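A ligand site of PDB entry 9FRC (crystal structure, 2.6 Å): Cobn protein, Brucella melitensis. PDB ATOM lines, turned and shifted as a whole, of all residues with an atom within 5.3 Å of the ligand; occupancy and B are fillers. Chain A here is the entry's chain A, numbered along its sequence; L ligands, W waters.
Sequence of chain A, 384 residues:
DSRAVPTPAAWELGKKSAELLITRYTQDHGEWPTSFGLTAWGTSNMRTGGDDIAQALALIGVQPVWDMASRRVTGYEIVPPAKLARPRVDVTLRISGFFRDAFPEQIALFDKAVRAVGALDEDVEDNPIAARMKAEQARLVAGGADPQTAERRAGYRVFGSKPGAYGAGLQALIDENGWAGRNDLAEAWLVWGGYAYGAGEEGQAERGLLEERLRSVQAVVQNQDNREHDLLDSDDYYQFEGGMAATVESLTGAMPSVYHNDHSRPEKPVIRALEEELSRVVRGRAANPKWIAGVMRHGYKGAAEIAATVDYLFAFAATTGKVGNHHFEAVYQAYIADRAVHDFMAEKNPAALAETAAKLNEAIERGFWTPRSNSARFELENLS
An oxygen (O11) of the ligand sits at hydrogen-bond distance from the side-chain hydroxyl (OG) of Ser 96 (2.6 Å).
The backbone NH (N) of Gly 97 lies within hydrogen-bond range of an oxygen (O9) of the ligand (2.7 Å).
The backbone NH (N) of Gly 42 lies within hydrogen-bond range of an oxygen (O11) of the ligand (2.8 Å).
The backbone NH (N) of Gly 167 is in hydrogen-bond range of an oxygen (O9) of the ligand.
An oxygen (O3) of the ligand lies within salt-bridge range of the guanidinium group (NH1) of Arg 47.
A ring nitrogen (NE2) of His 229 is in hydrogen-bond range of an oxygen (O2) of the ligand (2.8 Å).
N of Phe 98 is in hydrogen-bond range of O10 of the ligand.
The backbone NH of Thr 43 sits at hydrogen-bond distance from an oxygen (O12) of the ligand (3.1 Å).
An oxygen (O3) of the ligand is in hydrogen-bond range of the side-chain hydroxyl (OG1) of Thr 43 (3.1 Å).
OG of Ser 96 lies within hydrogen-bond range of N of Phe 99, 3.1 Å away.
OG1 of Thr 43 sits at hydrogen-bond distance from NH1 of Arg 47 (3.2 Å).
A ring nitrogen (ND1) of His 229 sits close to the side-chain hydroxyl (OH) of Tyr 237 (3.2 Å).
A ring nitrogen (NE2) of His 229 sits close to the side-chain amide oxygen of Asn 226, 3.4 Å away.
The side-chain carboxylate (OD2) of Asp 236 lies within hydrogen-bond range of the side-chain hydroxyl (OG) of Ser 234 (2.5 Å).
Merely in contact with the ligand: Asp 236, Trp 41, Phe 240, Tyr 166, Ser 234 and Phe 99.
Hydrophobic or aromatic side chains that line the ligand: Trp 41, Phe 98, Tyr 166, His 229 and Phe 240.
Within 4 Å of the ligand: Trp 41, Gly 42, Thr 43, Arg 47, Ser 96, Gly 97, Phe 98, Phe 99, Tyr 166, Gly 167, His 229, Ser 234, Asp 236 and Phe 240.
Water W1 lies within hydrogen-bond range of O of Gly 167, O9 of the ligand and OG of Ser 161.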
ATOM      1  N   TRP A  41      16.155   5.607 -20.453  1.00  0.00           N
ATOM      2  CA  TRP A  41      16.027   4.868 -19.210  1.00  0.00           C
ATOM      3  C   TRP A  41      16.434   3.416 -19.379  1.00  0.00           C
ATOM      4  O   TRP A  41      16.384   2.850 -20.462  1.00  0.00           O
ATOM      5  CB  TRP A  41      14.564   4.910 -18.758  1.00  0.00           C
ATOM      6  CG  TRP A  41      14.136   6.280 -18.332  1.00  0.00           C
ATOM      7  CD1 TRP A  41      14.932   7.367 -18.118  1.00  0.00           C
ATOM      8  CD2 TRP A  41      12.799   6.681 -17.965  1.00  0.00           C
ATOM      9  NE1 TRP A  41      14.185   8.416 -17.652  1.00  0.00           N
ATOM     10  CE2 TRP A  41      12.878   8.031 -17.550  1.00  0.00           C
ATOM     11  CE3 TRP A  41      11.556   6.033 -17.943  1.00  0.00           C
ATOM     12  CZ2 TRP A  41      11.756   8.744 -17.143  1.00  0.00           C
ATOM     13  CZ3 TRP A  41      10.454   6.752 -17.543  1.00  0.00           C
ATOM     14  CH2 TRP A  41      10.546   8.093 -17.144  1.00  0.00           C
ATOM     15  N   GLY A  42      16.714   2.796 -18.230  1.00  0.00           N
ATOM     16  CA  GLY A  42      17.298   1.472 -18.167  1.00  0.00           C
ATOM     17  C   GLY A  42      16.279   0.370 -18.443  1.00  0.00           C
ATOM     18  O   GLY A  42      16.505  -0.420 -19.344  1.00  0.00           O
ATOM     19  N   THR A  43      15.194   0.311 -17.654  1.00  0.00           N
ATOM     20  CA  THR A  43      14.271  -0.807 -17.708  1.00  0.00           C
ATOM     21  C   THR A  43      13.588  -0.834 -19.074  1.00  0.00           C
ATOM     22  O   THR A  43      13.288  -1.892 -19.599  1.00  0.00           O
ATOM     23  CB  THR A  43      13.233  -0.773 -16.587  1.00  0.00           C
ATOM     24  OG1 THR A  43      12.570   0.476 -16.775  1.00  0.00           O
ATOM     25  CG2 THR A  43      13.866  -0.830 -15.210  1.00  0.00           C
ATOM     26  N   SER A  44      13.382   0.362 -19.638  1.00  0.00           N
ATOM     27  CA  SER A  44      12.759   0.540 -20.928  1.00  0.00           C
ATOM     28  C   SER A  44      13.571  -0.170 -22.028  1.00  0.00           C
ATOM     29  O   SER A  44      13.022  -0.931 -22.816  1.00  0.00           O
ATOM     30  CB  SER A  44      12.590   2.018 -21.189  1.00  0.00           C
ATOM     31  OG  SER A  44      12.288   2.283 -22.553  1.00  0.00           O
ATOM     32  N   ARG A  47      13.480  -3.967 -21.881  1.00  0.00           N
ATOM     33  CA  ARG A  47      12.230  -4.551 -22.337  1.00  0.00           C
ATOM     34  C   ARG A  47      12.071  -4.541 -23.863  1.00  0.00           C
ATOM     35  O   ARG A  47      11.240  -5.281 -24.387  1.00  0.00           O
ATOM     36  CB  ARG A  47      11.066  -3.747 -21.753  1.00  0.00           C
ATOM     37  CG  ARG A  47      10.988  -3.800 -20.233  1.00  0.00           C
ATOM     38  CD  ARG A  47       9.576  -3.496 -19.708  1.00  0.00           C
ATOM     39  NE  ARG A  47       9.210  -2.087 -19.818  1.00  0.00           N
ATOM     40  CZ  ARG A  47       9.554  -1.105 -18.994  1.00  0.00           C
ATOM     41  NH1 ARG A  47      10.248  -1.355 -17.895  1.00  0.00           N
ATOM     42  NH2 ARG A  47       9.168   0.138 -19.255  1.00  0.00           N
ATOM     43  N   SER A  96      19.565   8.052 -17.572  1.00  0.00           N
ATOM     44  CA  SER A  96      19.249   7.905 -16.162  1.00  0.00           C
ATOM     45  C   SER A  96      20.404   7.188 -15.475  1.00  0.00           C
ATOM     46  O   SER A  96      21.265   6.620 -16.157  1.00  0.00           O
ATOM     47  CB  SER A  96      17.969   7.162 -16.016  1.00  0.00           C
ATOM     48  OG  SER A  96      18.170   5.798 -16.368  1.00  0.00           O
ATOM     49  N   GLY A  97      20.438   7.219 -14.146  1.00  0.00           N
ATOM     50  CA  GLY A  97      21.472   6.535 -13.391  1.00  0.00           C
ATOM     51  C   GLY A  97      21.486   5.020 -13.656  1.00  0.00           C
ATOM     52  O   GLY A  97      22.517   4.460 -14.007  1.00  0.00           O
ATOM     53  N   PHE A  98      20.345   4.365 -13.495  1.00  0.00           N
ATOM     54  CA  PHE A  98      20.214   2.966 -13.852  1.00  0.00           C
ATOM     55  C   PHE A  98      20.589   2.703 -15.325  1.00  0.00           C
ATOM     56  O   PHE A  98      21.091   1.627 -15.648  1.00  0.00           O
ATOM     57  CB  PHE A  98      18.794   2.536 -13.494  1.00  0.00           C
ATOM     58  CG  PHE A  98      18.551   1.057 -13.772  1.00  0.00           C
ATOM     59  CD1 PHE A  98      19.447   0.099 -13.312  1.00  0.00           C
ATOM     60  CD2 PHE A  98      17.471   0.645 -14.547  1.00  0.00           C
ATOM     61  CE1 PHE A  98      19.249  -1.243 -13.580  1.00  0.00           C
ATOM     62  CE2 PHE A  98      17.281  -0.698 -14.820  1.00  0.00           C
ATOM     63  CZ  PHE A  98      18.168  -1.639 -14.340  1.00  0.00           C
ATOM     64  N   PHE A  99      20.361   3.626 -16.262  1.00  0.00           N
ATOM     65  CA  PHE A  99      20.793   3.357 -17.628  1.00  0.00           C
ATOM     66  C   PHE A  99      22.327   3.414 -17.714  1.00  0.00           C
ATOM     67  O   PHE A  99      22.951   2.603 -18.407  1.00  0.00           O
ATOM     68  CB  PHE A  99      20.155   4.307 -18.646  1.00  0.00           C
ATOM     69  CG  PHE A  99      20.606   4.140 -20.091  1.00  0.00           C
ATOM     70  CD1 PHE A  99      21.797   4.679 -20.542  1.00  0.00           C
ATOM     71  CD2 PHE A  99      19.791   3.490 -21.009  1.00  0.00           C
ATOM     72  CE1 PHE A  99      22.196   4.559 -21.873  1.00  0.00           C
ATOM     73  CE2 PHE A  99      20.186   3.364 -22.328  1.00  0.00           C
ATOM     74  CZ  PHE A  99      21.400   3.878 -22.756  1.00  0.00           C
ATOM     75  N   SER A 161      23.406  12.116 -14.424  1.00  0.00           N
ATOM     76  CA  SER A 161      23.733  12.426 -13.042  1.00  0.00           C
ATOM     77  C   SER A 161      25.116  11.841 -12.742  1.00  0.00           C
ATOM     78  O   SER A 161      25.590  10.962 -13.469  1.00  0.00           O
ATOM     79  CB  SER A 161      22.689  11.876 -12.147  1.00  0.00           C
ATOM     80  OG  SER A 161      22.703  10.458 -12.297  1.00  0.00           O
ATOM     81  N   ALA A 165      25.028   8.445  -8.297  1.00  0.00           N
ATOM     82  CA  ALA A 165      23.764   9.146  -8.068  1.00  0.00           C
ATOM     83  C   ALA A 165      22.712   8.770  -9.116  1.00  0.00           C
ATOM     84  O   ALA A 165      23.029   8.234 -10.176  1.00  0.00           O
ATOM     85  CB  ALA A 165      24.016  10.636  -8.090  1.00  0.00           C
ATOM     86  N   TYR A 166      21.466   9.119  -8.803  1.00  0.00           N
ATOM     87  CA  TYR A 166      20.297   8.775  -9.597  1.00  0.00           C
ATOM     88  C   TYR A 166      19.340   9.955  -9.637  1.00  0.00           C
ATOM     89  O   TYR A 166      19.481  10.889  -8.859  1.00  0.00           O
ATOM     90  CB  TYR A 166      19.646   7.549  -8.944  1.00  0.00           C
ATOM     91  CG  TYR A 166      20.601   6.367  -8.962  1.00  0.00           C
ATOM     92  CD1 TYR A 166      21.530   6.196  -7.938  1.00  0.00           C
ATOM     93  CD2 TYR A 166      20.619   5.480 -10.035  1.00  0.00           C
ATOM     94  CE1 TYR A 166      22.432   5.149  -7.967  1.00  0.00           C
ATOM     95  CE2 TYR A 166      21.526   4.438 -10.077  1.00  0.00           C
ATOM     96  CZ  TYR A 166      22.438   4.283  -9.044  1.00  0.00           C
ATOM     97  OH  TYR A 166      23.360   3.289  -9.052  1.00  0.00           O
ATOM     98  N   GLY A 167      18.363   9.890 -10.568  1.00  0.00           N
ATOM     99  CA  GLY A 167      17.229  10.794 -10.594  1.00  0.00           C
ATOM    100  C   GLY A 167      17.545  12.050 -11.396  1.00  0.00           C
ATOM    101  O   GLY A 167      18.578  12.158 -12.054  1.00  0.00           O
ATOM    102  N   ASN A 226       5.521   0.897 -22.944  1.00  0.00           N
ATOM    103  CA  ASN A 226       4.423   0.101 -22.439  1.00  0.00           C
ATOM    104  C   ASN A 226       3.259   0.992 -21.997  1.00  0.00           C
ATOM    105  O   ASN A 226       3.446   2.146 -21.642  1.00  0.00           O
ATOM    106  CB  ASN A 226       4.866  -0.824 -21.320  1.00  0.00           C
ATOM    107  CG  ASN A 226       5.201  -0.067 -20.053  1.00  0.00           C
ATOM    108  OD1 ASN A 226       5.503   1.130 -20.117  1.00  0.00           O
ATOM    109  ND2 ASN A 226       5.133  -0.736 -18.912  1.00  0.00           N
ATOM    110  N   HIS A 229       2.160   2.172 -17.272  1.00  0.00           N
ATOM    111  CA  HIS A 229       2.145   3.507 -16.689  1.00  0.00           C
ATOM    112  C   HIS A 229       1.812   4.512 -17.799  1.00  0.00           C
ATOM    113  O   HIS A 229       1.609   4.151 -18.948  1.00  0.00           O
ATOM    114  CB  HIS A 229       3.394   3.787 -15.836  1.00  0.00           C
ATOM    115  CG  HIS A 229       4.679   3.408 -16.488  1.00  0.00           C
ATOM    116  ND1 HIS A 229       5.159   4.040 -17.616  1.00  0.00           N
ATOM    117  CD2 HIS A 229       5.543   2.431 -16.201  1.00  0.00           C
ATOM    118  CE1 HIS A 229       6.300   3.470 -17.980  1.00  0.00           C
ATOM    119  NE2 HIS A 229       6.547   2.489 -17.133  1.00  0.00           N
ATOM    120  N   SER A 234       3.170   9.103 -12.573  1.00  0.00           N
ATOM    121  CA  SER A 234       4.493   9.026 -11.990  1.00  0.00           C
ATOM    122  C   SER A 234       5.194  10.369 -12.164  1.00  0.00           C
ATOM    123  O   SER A 234       4.896  11.114 -13.105  1.00  0.00           O
ATOM    124  CB  SER A 234       5.269   7.898 -12.601  1.00  0.00           C
ATOM    125  OG  SER A 234       6.658   8.088 -12.472  1.00  0.00           O
ATOM    126  N   ASP A 236       8.301  10.796 -12.804  1.00  0.00           N
ATOM    127  CA  ASP A 236       9.528  10.595 -13.555  1.00  0.00           C
ATOM    128  C   ASP A 236       9.517  11.295 -14.913  1.00  0.00           C
ATOM    129  O   ASP A 236      10.559  11.781 -15.342  1.00  0.00           O
ATOM    130  CB  ASP A 236       9.805   9.098 -13.603  1.00  0.00           C
ATOM    131  CG  ASP A 236       9.919   8.450 -12.227  1.00  0.00           C
ATOM    132  OD1 ASP A 236      10.864   8.811 -11.465  1.00  0.00           O
ATOM    133  OD2 ASP A 236       9.038   7.611 -11.896  1.00  0.00           O
ATOM    134  N   TYR A 237       8.365  11.362 -15.600  1.00  0.00           N
ATOM    135  CA  TYR A 237       8.288  11.816 -16.981  1.00  0.00           C
ATOM    136  C   TYR A 237       8.497  13.337 -17.038  1.00  0.00           C
ATOM    137  O   TYR A 237       9.238  13.852 -17.896  1.00  0.00           O
ATOM    138  CB  TYR A 237       6.963  11.377 -17.613  1.00  0.00           C
ATOM    139  CG  TYR A 237       6.966   9.933 -18.069  1.00  0.00           C
ATOM    140  CD1 TYR A 237       7.508   9.586 -19.291  1.00  0.00           C
ATOM    141  CD2 TYR A 237       6.406   8.918 -17.293  1.00  0.00           C
ATOM    142  CE1 TYR A 237       7.544   8.261 -19.718  1.00  0.00           C
ATOM    143  CE2 TYR A 237       6.425   7.595 -17.709  1.00  0.00           C
ATOM    144  CZ  TYR A 237       7.004   7.271 -18.916  1.00  0.00           C
ATOM    145  OH  TYR A 237       7.044   5.991 -19.379  1.00  0.00           O
ATOM    146  N   PHE A 240      12.220  14.269 -16.270  1.00  0.00           N
ATOM    147  CA  PHE A 240      13.186  13.996 -17.316  1.00  0.00           C
ATOM    148  C   PHE A 240      12.877  14.832 -18.546  1.00  0.00           C
ATOM    149  O   PHE A 240      13.745  15.612 -18.979  1.00  0.00           O
ATOM    150  CB  PHE A 240      13.291  12.491 -17.608  1.00  0.00           C
ATOM    151  CG  PHE A 240      14.299  11.871 -16.665  1.00  0.00           C
ATOM    152  CD1 PHE A 240      13.946  11.520 -15.372  1.00  0.00           C
ATOM    153  CD2 PHE A 240      15.622  11.724 -17.060  1.00  0.00           C
ATOM    154  CE1 PHE A 240      14.875  10.989 -14.509  1.00  0.00           C
ATOM    155  CE2 PHE A 240      16.546  11.218 -16.172  1.00  0.00           C
ATOM    156  CZ  PHE A 240      16.169  10.848 -14.911  1.00  0.00           C
HETATM  157  C1  LIG L   1      11.878   5.518 -13.028  1.00  0.00           C
HETATM  158  C2  LIG L   1      10.833   4.769 -12.541  1.00  0.00           C
HETATM  159  C3  LIG L   1       9.494   4.505 -13.241  1.00  0.00           C
HETATM  160  C4  LIG L   1       8.632   3.747 -12.198  1.00  0.00           C
HETATM  161  C5  LIG L   1       9.524   3.950 -10.981  1.00  0.00           C
HETATM  162  C6  LIG L   1       9.033   3.794  -9.727  1.00  0.00           C
HETATM  163  O1  LIG L   1      15.877   0.583  -4.919  1.00  0.00           O
HETATM  164  O2  LIG L   1       9.391   2.640 -17.160  1.00  0.00           O
HETATM  165  C7  LIG L   1       9.728   1.959 -16.169  1.00  0.00           C
HETATM  166  O3  LIG L   1       9.572   0.709 -16.075  1.00  0.00           O
HETATM  167  C8  LIG L   1      10.340   2.708 -14.992  1.00  0.00           C
HETATM  168  C9  LIG L   1       9.395   3.848 -14.639  1.00  0.00           C
HETATM  169  C10 LIG L   1       8.330   2.252 -12.398  1.00  0.00           C
HETATM  170  C11 LIG L   1       7.298   4.519 -12.069  1.00  0.00           C
HETATM  171  N1  LIG L   1      10.791   4.283 -11.281  1.00  0.00           N
HETATM  172  C12 LIG L   1       9.662   3.164  -8.683  1.00  0.00           C
HETATM  173  N2  LIG L   1      11.012   3.086  -8.479  1.00  0.00           N
HETATM  174  C13 LIG L   1      11.225   3.206  -7.130  1.00  0.00           C
HETATM  175  C14 LIG L   1      10.047   2.500  -6.414  1.00  0.00           C
HETATM  176  C15 LIG L   1      10.477   1.102  -5.953  1.00  0.00           C
HETATM  177  C16 LIG L   1       9.441   3.302  -5.217  1.00  0.00           C
HETATM  178  C17 LIG L   1       8.879   4.683  -5.474  1.00  0.00           C
HETATM  179  N3  LIG L   1       7.558   4.794  -5.548  1.00  0.00           N
HETATM  180  O4  LIG L   1       9.631   5.656  -5.583  1.00  0.00           O
HETATM  181  C18 LIG L   1       8.953   2.479  -7.530  1.00  0.00           C
HETATM  182  C19 LIG L   1       8.433   1.084  -7.968  1.00  0.00           C
HETATM  183  C20 LIG L   1       7.254   1.068  -8.959  1.00  0.00           C
HETATM  184  C21 LIG L   1       5.865   1.391  -8.401  1.00  0.00           C
HETATM  185  O5  LIG L   1       4.892   1.276  -9.189  1.00  0.00           O
HETATM  186  O6  LIG L   1       5.752   1.754  -7.203  1.00  0.00           O
HETATM  187  C22 LIG L   1      12.420   3.793  -6.612  1.00  0.00           C
HETATM  188  C23 LIG L   1      12.637   3.949  -5.116  1.00  0.00           C
HETATM  189  C24 LIG L   1      13.442   4.189  -7.443  1.00  0.00           C
HETATM  190  C25 LIG L   1      14.913   4.260  -7.060  1.00  0.00           C
HETATM  191  C26 LIG L   1      15.516   2.850  -6.808  1.00  0.00           C
HETATM  192  C27 LIG L   1      16.435   2.803  -5.582  1.00  0.00           C
HETATM  193  C28 LIG L   1      16.810   1.419  -5.078  1.00  0.00           C
HETATM  194  O7  LIG L   1      18.027   1.180  -4.813  1.00  0.00           O
HETATM  195  C29 LIG L   1      15.524   5.149  -8.195  1.00  0.00           C
HETATM  196  C30 LIG L   1      17.009   4.858  -8.445  1.00  0.00           C
HETATM  197  C31 LIG L   1      15.330   6.640  -7.763  1.00  0.00           C
HETATM  198  C32 LIG L   1      16.347   7.210  -6.798  1.00  0.00           C
HETATM  199  N4  LIG L   1      16.950   6.379  -5.946  1.00  0.00           N
HETATM  200  O8  LIG L   1      16.611   8.423  -6.812  1.00  0.00           O
HETATM  201  C33 LIG L   1      14.579   4.757  -9.390  1.00  0.00           C
HETATM  202  N5  LIG L   1      13.287   4.553  -8.672  1.00  0.00           N
HETATM  203  C34 LIG L   1      14.859   3.433 -10.084  1.00  0.00           C
HETATM  204  C35 LIG L   1      14.313   5.854 -10.413  1.00  0.00           C
HETATM  205  N6  LIG L   1      13.057   5.420 -11.050  1.00  0.00           N
HETATM  206  C36 LIG L   1      13.029   5.772 -12.303  1.00  0.00           C
HETATM  207  C37 LIG L   1      11.741   6.091 -14.429  1.00  0.00           C
HETATM  208  C38 LIG L   1      14.379   6.391 -12.743  1.00  0.00           C
HETATM  209  C39 LIG L   1      14.246   7.900 -13.025  1.00  0.00           C
HETATM  210  C40 LIG L   1      15.327   6.090 -11.541  1.00  0.00           C
HETATM  211  C41 LIG L   1      16.496   7.068 -11.271  1.00  0.00           C
HETATM  212  C42 LIG L   1      17.724   6.852 -12.166  1.00  0.00           C
HETATM  213  O9  LIG L   1      18.469   7.820 -12.450  1.00  0.00           O
HETATM  214  O10 LIG L   1      17.979   5.714 -12.580  1.00  0.00           O
HETATM  215  C43 LIG L   1      14.922   5.694 -14.000  1.00  0.00           C
HETATM  216  C44 LIG L   1      14.894   4.167 -13.977  1.00  0.00           C
HETATM  217  C45 LIG L   1      15.353   3.542 -15.281  1.00  0.00           C
HETATM  218  O11 LIG L   1      16.485   3.898 -15.717  1.00  0.00           O
HETATM  219  O12 LIG L   1      14.592   2.705 -15.830  1.00  0.00           O
HETATM  220  O   HOH W   1      19.682  10.636 -13.822  1.00  0.00           O
